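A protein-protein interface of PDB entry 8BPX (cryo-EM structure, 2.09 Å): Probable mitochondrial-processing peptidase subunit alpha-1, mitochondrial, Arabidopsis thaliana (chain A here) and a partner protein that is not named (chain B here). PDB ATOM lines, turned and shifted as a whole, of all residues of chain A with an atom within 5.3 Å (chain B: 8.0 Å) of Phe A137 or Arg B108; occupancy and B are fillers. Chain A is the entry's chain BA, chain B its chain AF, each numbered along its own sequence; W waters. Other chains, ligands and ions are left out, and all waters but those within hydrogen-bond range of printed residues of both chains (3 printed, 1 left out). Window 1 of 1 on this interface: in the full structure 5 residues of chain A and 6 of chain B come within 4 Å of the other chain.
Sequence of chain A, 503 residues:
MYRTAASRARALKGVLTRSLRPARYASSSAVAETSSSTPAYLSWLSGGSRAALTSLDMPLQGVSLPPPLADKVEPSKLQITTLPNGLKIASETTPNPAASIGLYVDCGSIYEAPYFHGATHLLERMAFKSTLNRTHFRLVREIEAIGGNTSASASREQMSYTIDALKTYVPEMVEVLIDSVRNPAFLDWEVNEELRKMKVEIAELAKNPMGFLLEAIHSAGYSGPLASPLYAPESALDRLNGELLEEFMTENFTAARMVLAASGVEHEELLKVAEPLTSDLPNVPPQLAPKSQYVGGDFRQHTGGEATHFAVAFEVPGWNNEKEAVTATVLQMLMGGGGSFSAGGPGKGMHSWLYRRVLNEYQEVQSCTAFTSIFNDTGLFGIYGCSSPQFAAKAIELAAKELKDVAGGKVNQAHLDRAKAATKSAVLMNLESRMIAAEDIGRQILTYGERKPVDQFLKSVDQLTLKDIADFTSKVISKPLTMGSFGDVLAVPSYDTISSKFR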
ATOM      1  N   THR A 135      13.412  -9.478  -4.088  1.00  0.00           N
ATOM      2  CA  THR A 135      14.544  -8.980  -4.848  1.00  0.00           C
ATOM      3  C   THR A 135      15.828  -9.131  -4.044  1.00  0.00           C
ATOM      4  O   THR A 135      15.805  -9.322  -2.825  1.00  0.00           O
ATOM      5  CB  THR A 135      14.338  -7.511  -5.217  1.00  0.00           C
ATOM      6  OG1 THR A 135      14.209  -6.732  -4.023  1.00  0.00           O
ATOM      7  CG2 THR A 135      13.081  -7.349  -6.057  1.00  0.00           C
ATOM      8  N   HIS A 136      16.956  -9.050  -4.746  1.00  0.00           N
ATOM      9  CA  HIS A 136      18.253  -9.027  -4.084  1.00  0.00           C
ATOM     10  C   HIS A 136      18.330  -7.881  -3.078  1.00  0.00           C
ATOM     11  O   HIS A 136      18.851  -8.040  -1.967  1.00  0.00           O
ATOM     12  CB  HIS A 136      19.355  -8.918  -5.140  1.00  0.00           C
ATOM     13  CG  HIS A 136      20.745  -9.012  -4.592  1.00  0.00           C
ATOM     14  ND1 HIS A 136      21.852  -8.622  -5.312  1.00  0.00           N
ATOM     15  CD2 HIS A 136      21.207  -9.453  -3.399  1.00  0.00           C
ATOM     16  CE1 HIS A 136      22.936  -8.817  -4.586  1.00  0.00           C
ATOM     17  NE2 HIS A 136      22.573  -9.320  -3.421  1.00  0.00           N
ATOM     18  N   PHE A 137      17.789  -6.718  -3.450  1.00  0.00           N
ATOM     19  CA  PHE A 137      17.811  -5.559  -2.566  1.00  0.00           C
ATOM     20  C   PHE A 137      17.062  -5.838  -1.267  1.00  0.00           C
ATOM     21  O   PHE A 137      17.563  -5.556  -0.172  1.00  0.00           O
ATOM     22  CB  PHE A 137      17.217  -4.347  -3.289  1.00  0.00           C
ATOM     23  CG  PHE A 137      16.962  -3.174  -2.393  1.00  0.00           C
ATOM     24  CD1 PHE A 137      18.014  -2.413  -1.908  1.00  0.00           C
ATOM     25  CD2 PHE A 137      15.671  -2.833  -2.033  1.00  0.00           C
ATOM     26  CE1 PHE A 137      17.783  -1.333  -1.079  1.00  0.00           C
ATOM     27  CE2 PHE A 137      15.433  -1.754  -1.209  1.00  0.00           C
ATOM     28  CZ  PHE A 137      16.491  -1.002  -0.728  1.00  0.00           C
ATOM     29  N   ARG A 138      15.863  -6.413  -1.370  1.00  0.00           N
ATOM     30  CA  ARG A 138      15.089  -6.688  -0.167  1.00  0.00           C
ATOM     31  C   ARG A 138      15.741  -7.781   0.672  1.00  0.00           C
ATOM     32  O   ARG A 138      15.682  -7.738   1.903  1.00  0.00           O
ATOM     33  CB  ARG A 138      13.652  -7.059  -0.529  1.00  0.00           C
ATOM     34  CG  ARG A 138      12.819  -7.456   0.673  1.00  0.00           C
ATOM     35  CD  ARG A 138      11.460  -7.989   0.295  1.00  0.00           C
ATOM     36  NE  ARG A 138      10.888  -8.785   1.371  1.00  0.00           N
ATOM     37  CZ  ARG A 138       9.855  -8.409   2.114  1.00  0.00           C
ATOM     38  NH1 ARG A 138       9.257  -7.246   1.926  1.00  0.00           N
ATOM     39  NH2 ARG A 138       9.417  -9.221   3.072  1.00  0.00           N
ATOM     40  N   LEU A 139      16.380  -8.758   0.028  1.00  0.00           N
ATOM     41  CA  LEU A 139      17.097  -9.793   0.769  1.00  0.00           C
ATOM     42  C   LEU A 139      18.241  -9.198   1.585  1.00  0.00           C
ATOM     43  O   LEU A 139      18.391  -9.490   2.779  1.00  0.00           O
ATOM     44  CB  LEU A 139      17.620 -10.848  -0.203  1.00  0.00           C
ATOM     45  CG  LEU A 139      18.139 -12.157   0.386  1.00  0.00           C
ATOM     46  CD1 LEU A 139      17.061 -12.803   1.224  1.00  0.00           C
ATOM     47  CD2 LEU A 139      18.575 -13.088  -0.723  1.00  0.00           C
ATOM     48  N   VAL A 140      19.055  -8.353   0.946  1.00  0.00           N
ATOM     49  CA  VAL A 140      20.158  -7.711   1.651  1.00  0.00           C
ATOM     50  C   VAL A 140      19.633  -6.860   2.797  1.00  0.00           C
ATOM     51  O   VAL A 140      20.186  -6.877   3.903  1.00  0.00           O
ATOM     52  CB  VAL A 140      21.019  -6.889   0.674  1.00  0.00           C
ATOM     53  CG1 VAL A 140      22.030  -6.031   1.430  1.00  0.00           C
ATOM     54  CG2 VAL A 140      21.728  -7.806  -0.303  1.00  0.00           C
ATOM     55  N   ARG A 141      18.549  -6.116   2.563  1.00  0.00           N
ATOM     56  CA  ARG A 141      18.005  -5.276   3.625  1.00  0.00           C
ATOM     57  C   ARG A 141      17.447  -6.112   4.773  1.00  0.00           C
ATOM     58  O   ARG A 141      17.595  -5.741   5.941  1.00  0.00           O
ATOM     59  CB  ARG A 141      16.949  -4.331   3.058  1.00  0.00           C
ATOM     60  CG  ARG A 141      17.548  -3.148   2.310  1.00  0.00           C
ATOM     61  CD  ARG A 141      18.623  -2.462   3.143  1.00  0.00           C
ATOM     62  NE  ARG A 141      19.340  -1.433   2.400  1.00  0.00           N
ATOM     63  CZ  ARG A 141      18.965  -0.163   2.326  1.00  0.00           C
ATOM     64  NH1 ARG A 141      17.870   0.270   2.924  1.00  0.00           N
ATOM     65  NH2 ARG A 141      19.709   0.692   1.635  1.00  0.00           N
ATOM     66  N   GLU A 142      16.813  -7.248   4.464  1.00  0.00           N
ATOM     67  CA  GLU A 142      16.309  -8.128   5.513  1.00  0.00           C
ATOM     68  C   GLU A 142      17.444  -8.674   6.368  1.00  0.00           C
ATOM     69  O   GLU A 142      17.343  -8.701   7.598  1.00  0.00           O
ATOM     70  CB  GLU A 142      15.508  -9.281   4.903  1.00  0.00           C
ATOM     71  CG  GLU A 142      14.095  -8.922   4.475  1.00  0.00           C
ATOM     72  CD  GLU A 142      13.532  -9.887   3.447  1.00  0.00           C
ATOM     73  OE1 GLU A 142      14.322 -10.473   2.677  1.00  0.00           O
ATOM     74  OE2 GLU A 142      12.297 -10.059   3.406  1.00  0.00           O
ATOM     75  N   VAL B 101      11.170  -2.636 -13.663  1.00  0.00           N
ATOM     76  CA  VAL B 101      12.187  -1.651 -13.300  1.00  0.00           C
ATOM     77  C   VAL B 101      11.590  -0.564 -12.413  1.00  0.00           C
ATOM     78  O   VAL B 101      12.183  -0.169 -11.399  1.00  0.00           O
ATOM     79  CB  VAL B 101      12.827  -1.063 -14.572  1.00  0.00           C
ATOM     80  CG1 VAL B 101      13.681   0.137 -14.240  1.00  0.00           C
ATOM     81  CG2 VAL B 101      13.660  -2.115 -15.278  1.00  0.00           C
ATOM     82  N   LYS B 102      10.406  -0.066 -12.777  1.00  0.00           N
ATOM     83  CA  LYS B 102       9.770   0.980 -11.983  1.00  0.00           C
ATOM     84  C   LYS B 102       9.402   0.474 -10.593  1.00  0.00           C
ATOM     85  O   LYS B 102       9.547   1.202  -9.603  1.00  0.00           O
ATOM     86  CB  LYS B 102       8.542   1.525 -12.711  1.00  0.00           C
ATOM     87  CG  LYS B 102       8.885   2.397 -13.903  1.00  0.00           C
ATOM     88  CD  LYS B 102       7.833   2.301 -14.986  1.00  0.00           C
ATOM     89  CE  LYS B 102       7.843   3.526 -15.886  1.00  0.00           C
ATOM     90  NZ  LYS B 102       9.135   4.270 -15.842  1.00  0.00           N
ATOM     91  N   ARG B 103       8.930  -0.771 -10.496  1.00  0.00           N
ATOM     92  CA  ARG B 103       8.626  -1.345  -9.186  1.00  0.00           C
ATOM     93  C   ARG B 103       9.882  -1.455  -8.328  1.00  0.00           C
ATOM     94  O   ARG B 103       9.848  -1.167  -7.126  1.00  0.00           O
ATOM     95  CB  ARG B 103       7.967  -2.715  -9.348  1.00  0.00           C
ATOM     96  CG  ARG B 103       6.483  -2.664  -9.653  1.00  0.00           C
ATOM     97  CD  ARG B 103       5.810  -4.003  -9.397  1.00  0.00           C
ATOM     98  NE  ARG B 103       6.269  -5.046 -10.303  1.00  0.00           N
ATOM     99  CZ  ARG B 103       5.975  -5.112 -11.595  1.00  0.00           C
ATOM    100  NH1 ARG B 103       5.182  -4.224 -12.172  1.00  0.00           N
ATOM    101  NH2 ARG B 103       6.487  -6.097 -12.325  1.00  0.00           N
ATOM    102  N   GLU B 104      10.998  -1.870  -8.929  1.00  0.00           N
ATOM    103  CA  GLU B 104      12.247  -1.975  -8.178  1.00  0.00           C
ATOM    104  C   GLU B 104      12.722  -0.609  -7.689  1.00  0.00           C
ATOM    105  O   GLU B 104      13.188  -0.476  -6.548  1.00  0.00           O
ATOM    106  CB  GLU B 104      13.312  -2.654  -9.038  1.00  0.00           C
ATOM    107  CG  GLU B 104      13.018  -4.124  -9.312  1.00  0.00           C
ATOM    108  CD  GLU B 104      14.047  -4.775 -10.215  1.00  0.00           C
ATOM    109  OE1 GLU B 104      14.063  -6.019 -10.303  1.00  0.00           O
ATOM    110  OE2 GLU B 104      14.837  -4.041 -10.841  1.00  0.00           O
ATOM    111  N   ARG B 105      12.607   0.420  -8.532  1.00  0.00           N
ATOM    112  CA  ARG B 105      12.993   1.761  -8.097  1.00  0.00           C
ATOM    113  C   ARG B 105      12.091   2.267  -6.978  1.00  0.00           C
ATOM    114  O   ARG B 105      12.564   2.915  -6.037  1.00  0.00           O
ATOM    115  CB  ARG B 105      12.985   2.735  -9.275  1.00  0.00           C
ATOM    116  CG  ARG B 105      14.352   2.946  -9.911  1.00  0.00           C
ATOM    117  CD  ARG B 105      15.405   3.518  -8.936  1.00  0.00           C
ATOM    118  NE  ARG B 105      14.854   4.402  -7.911  1.00  0.00           N
ATOM    119  CZ  ARG B 105      14.573   5.685  -8.103  1.00  0.00           C
ATOM    120  NH1 ARG B 105      14.768   6.270  -9.272  1.00  0.00           N
ATOM    121  NH2 ARG B 105      14.085   6.399  -7.091  1.00  0.00           N
ATOM    122  N   ALA B 106      10.786   1.987  -7.065  1.00  0.00           N
ATOM    123  CA  ALA B 106       9.878   2.375  -5.990  1.00  0.00           C
ATOM    124  C   ALA B 106      10.237   1.668  -4.690  1.00  0.00           C
ATOM    125  O   ALA B 106      10.182   2.269  -3.612  1.00  0.00           O
ATOM    126  CB  ALA B 106       8.432   2.078  -6.383  1.00  0.00           C
ATOM    127  N   GLU B 107      10.609   0.389  -4.773  1.00  0.00           N
ATOM    128  CA  GLU B 107      11.033  -0.331  -3.579  1.00  0.00           C
ATOM    129  C   GLU B 107      12.281   0.301  -2.973  1.00  0.00           C
ATOM    130  O   GLU B 107      12.368   0.470  -1.752  1.00  0.00           O
ATOM    131  CB  GLU B 107      11.286  -1.803  -3.909  1.00  0.00           C
ATOM    132  CG  GLU B 107      11.491  -2.677  -2.684  1.00  0.00           C
ATOM    133  CD  GLU B 107      11.987  -4.074  -3.020  1.00  0.00           C
ATOM    134  OE1 GLU B 107      12.579  -4.265  -4.102  1.00  0.00           O
ATOM    135  OE2 GLU B 107      11.778  -4.987  -2.197  1.00  0.00           O
ATOM    136  N   ARG B 108      13.253   0.665  -3.814  1.00  0.00           N
ATOM    137  CA  ARG B 108      14.464   1.306  -3.312  1.00  0.00           C
ATOM    138  C   ARG B 108      14.152   2.630  -2.627  1.00  0.00           C
ATOM    139  O   ARG B 108      14.702   2.932  -1.563  1.00  0.00           O
ATOM    140  CB  ARG B 108      15.460   1.523  -4.448  1.00  0.00           C
ATOM    141  CG  ARG B 108      16.033   0.252  -5.021  1.00  0.00           C
ATOM    142  CD  ARG B 108      17.291   0.520  -5.815  1.00  0.00           C
ATOM    143  NE  ARG B 108      18.341   1.126  -5.007  1.00  0.00           N
ATOM    144  CZ  ARG B 108      19.368   0.457  -4.504  1.00  0.00           C
ATOM    145  NH1 ARG B 108      19.489  -0.848  -4.673  1.00  0.00           N
ATOM    146  NH2 ARG B 108      20.292   1.113  -3.812  1.00  0.00           N
ATOM    147  N   GLU B 109      13.272   3.436  -3.227  1.00  0.00           N
ATOM    148  CA  GLU B 109      12.929   4.725  -2.630  1.00  0.00           C
ATOM    149  C   GLU B 109      12.176   4.546  -1.317  1.00  0.00           C
ATOM    150  O   GLU B 109      12.396   5.298  -0.362  1.00  0.00           O
ATOM    151  CB  GLU B 109      12.115   5.562  -3.614  1.00  0.00           C
ATOM    152  CG  GLU B 109      11.785   6.962  -3.132  1.00  0.00           C
ATOM    153  CD  GLU B 109      12.992   7.697  -2.573  1.00  0.00           C
ATOM    154  OE1 GLU B 109      13.823   8.173  -3.374  1.00  0.00           O
ATOM    155  OE2 GLU B 109      13.105   7.812  -1.333  1.00  0.00           O
ATOM    156  N   ALA B 110      11.288   3.551  -1.247  1.00  0.00           N
ATOM    157  CA  ALA B 110      10.502   3.324  -0.040  1.00  0.00           C
ATOM    158  C   ALA B 110      11.352   2.879   1.145  1.00  0.00           C
ATOM    159  O   ALA B 110      10.917   3.027   2.291  1.00  0.00           O
ATOM    160  CB  ALA B 110       9.416   2.285  -0.311  1.00  0.00           C
ATOM    161  N   LEU B 111      12.541   2.331   0.905  1.00  0.00           N
ATOM    162  CA  LEU B 111      13.425   1.900   1.977  1.00  0.00           C
ATOM    163  C   LEU B 111      14.571   2.874   2.224  1.00  0.00           C
ATOM    164  O   LEU B 111      15.461   2.576   3.023  1.00  0.00           O
ATOM    165  CB  LEU B 111      13.970   0.503   1.679  1.00  0.00           C
ATOM    166  CG  LEU B 111      12.987  -0.661   1.826  1.00  0.00           C
ATOM    167  CD1 LEU B 111      13.718  -1.989   1.782  1.00  0.00           C
ATOM    168  CD2 LEU B 111      12.194  -0.540   3.108  1.00  0.00           C
ATOM    169  N   GLY B 112      14.568   4.028   1.560  1.00  0.00           N
ATOM    170  CA  GLY B 112      15.581   5.039   1.796  1.00  0.00           C
ATOM    171  C   GLY B 112      16.918   4.794   1.139  1.00  0.00           C
ATOM    172  O   GLY B 112      17.915   5.391   1.552  1.00  0.00           O
ATOM    173  N   ALA B 113      16.973   3.936   0.126  1.00  0.00           N
ATOM    174  CA  ALA B 113      18.220   3.623  -0.550  1.00  0.00           C
ATOM    175  C   ALA B 113      18.546   4.665  -1.617  1.00  0.00           C
ATOM    176  O   ALA B 113      17.689   5.424  -2.071  1.00  0.00           O
ATOM    177  CB  ALA B 113      18.148   2.234  -1.184  1.00  0.00           C
ATOM    178  N   LEU B 114      19.812   4.693  -2.009  1.00  0.00           N
ATOM    179  CA  LEU B 114      20.229   5.534  -3.118  1.00  0.00           C
ATOM    180  C   LEU B 114      19.721   4.947  -4.435  1.00  0.00           C
ATOM    181  O   LEU B 114      19.682   3.726  -4.595  1.00  0.00           O
ATOM    182  CB  LEU B 114      21.751   5.653  -3.152  1.00  0.00           C
ATOM    183  CG  LEU B 114      22.427   6.475  -2.049  1.00  0.00           C
ATOM    184  CD1 LEU B 114      23.784   6.974  -2.515  1.00  0.00           C
ATOM    185  CD2 LEU B 114      21.549   7.644  -1.626  1.00  0.00           C
ATOM    186  N   PRO B 115      19.321   5.787  -5.388  1.00  0.00           N
ATOM    187  CA  PRO B 115      18.906   5.267  -6.697  1.00  0.00           C
ATOM    188  C   PRO B 115      20.057   4.576  -7.414  1.00  0.00           C
ATOM    189  O   PRO B 115      21.222   4.949  -7.273  1.00  0.00           O
ATOM    190  CB  PRO B 115      18.450   6.522  -7.449  1.00  0.00           C
ATOM    191  CG  PRO B 115      19.191   7.641  -6.777  1.00  0.00           C
ATOM    192  CD  PRO B 115      19.251   7.257  -5.333  1.00  0.00           C
ATOM    193  N   LEU B 116      19.712   3.547  -8.190  1.00  0.00           N
ATOM    194  CA  LEU B 116      20.719   2.781  -8.915  1.00  0.00           C
ATOM    195  C   LEU B 116      21.292   3.542 -10.101  1.00  0.00           C
ATOM    196  O   LEU B 116      22.383   3.204 -10.570  1.00  0.00           O
ATOM    197  CB  LEU B 116      20.125   1.457  -9.389  1.00  0.00           C
ATOM    198  CG  LEU B 116      20.067   0.326  -8.361  1.00  0.00           C
ATOM    199  CD1 LEU B 116      19.632  -0.964  -9.024  1.00  0.00           C
ATOM    200  CD2 LEU B 116      21.409   0.149  -7.666  1.00  0.00           C
ATOM    201  N   TYR B 117      20.581   4.548 -10.600  1.00  0.00           N
ATOM    202  CA  TYR B 117      21.049   5.365 -11.706  1.00  0.00           C
ATOM    203  C   TYR B 117      20.349   6.709 -11.626  1.00  0.00           C
ATOM    204  O   TYR B 117      19.247   6.824 -11.086  1.00  0.00           O
ATOM    205  CB  TYR B 117      20.794   4.687 -13.057  1.00  0.00           C
ATOM    206  CG  TYR B 117      19.434   4.045 -13.137  1.00  0.00           C
ATOM    207  CD1 TYR B 117      18.294   4.814 -13.317  1.00  0.00           C
ATOM    208  CD2 TYR B 117      19.285   2.675 -12.984  1.00  0.00           C
ATOM    209  CE1 TYR B 117      17.049   4.240 -13.369  1.00  0.00           C
ATOM    210  CE2 TYR B 117      18.040   2.089 -13.033  1.00  0.00           C
ATOM    211  CZ  TYR B 117      16.927   2.878 -13.225  1.00  0.00           C
ATOM    212  OH  TYR B 117      15.685   2.312 -13.279  1.00  0.00           O
HETATM  213  O   HOH W   1      20.606   0.139  -1.122  1.00  0.00           O
HETATM  214  O   HOH W   2      19.671   3.535   3.091  1.00  0.00           O
HETATM  215  O   HOH W   3      11.101  -7.639  -3.188  1.00  0.00           O
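The backbone carbonyl oxygen (O) of Leu B111 is in hydrogen-bond range of the guanidinium group (NH1) of Arg A141. The side-chain hydroxyl of Thr A135 is in hydrogen-bond range of the side-chain carboxylate of Glu B107 (3.0 Å).
Of the 8 printed residues of chain A, 4 touch a printed residue of chain B. Hydrophobic or aromatic side chains of chain A that line the printed part of chain B: Phe A137. Among the printed residues, no Asp or Glu carboxylate lies within 4 Å of a Lys or Arg side-chain nitrogen of the other chain.
Among the printed residues, pairs that only touch across the chains: Arg A138 with Glu B107, Phe A137 with Leu B111, Phe A137 with Arg B108, Arg A141 with Ala B113, Phe A137 with Ala B113 and Phe A137 with Glu B107.
Of the printed residues of chain B, Thr A135 touches Glu B107. Of the printed residues of chain B, Phe A137 touches Glu B107, Arg B108, Leu B111 and Ala B113. Printed residues of chain B within 4 Å of Arg A141: Leu B111 and Ala B113. Lys B102 touches none of the printed residues of chain A. Of the printed residues of chain A, Glu B107 touches Thr A135 (3.0 Å), Phe A137 (3.8 Å) and Arg A138 (3.3 Å). Of chain A, only Phe A137 comes within 4 Å of Arg B108. Of the printed residues of chain A, Leu B111 touches Phe A137 (3.5 Å) and Arg A141 (3.3 Å). Printed residues of chain A within 4 Å of Ala B113: Phe A137 (3.6 Å) and Arg A141 (3.6 Å). Leu B116 touches none of the printed residues of chain A. The nearest printed residue of chain A that does not touch Arg B108 is Arg A141 (5.5 Å). The nearest printed residue of chain A that does not touch Leu B111 is Arg A138 (5.3 Å).
The backbone NH (N) of Arg A138 sits at hydrogen-bond distance from the side-chain hydroxyl (OG1) of Thr A135, at 3.1 Å. The guanidinium group (NH2) of Arg B108 is in hydrogen-bond range of the backbone carbonyl oxygen (O) of Leu B114. N of Ala B113 is in hydrogen-bond range of O of Arg B108, at 3.0 Å. The guanidinium group of Arg A138 lies within salt-bridge range of the side-chain carboxylate of Glu A142, at 2.8 Å.
Water W1 lies within hydrogen-bond range of the guanidinium group of Arg B108 (2.9 Å) and the guanidinium group of Arg A141 (3.0 Å). Water W3 lies within hydrogen-bond range of the side-chain carboxylate (OE2) of Glu B107 and the backbone NH (N) of Thr A135. Water W2 bridges O of Gly B112 and NH2 of Arg A141.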
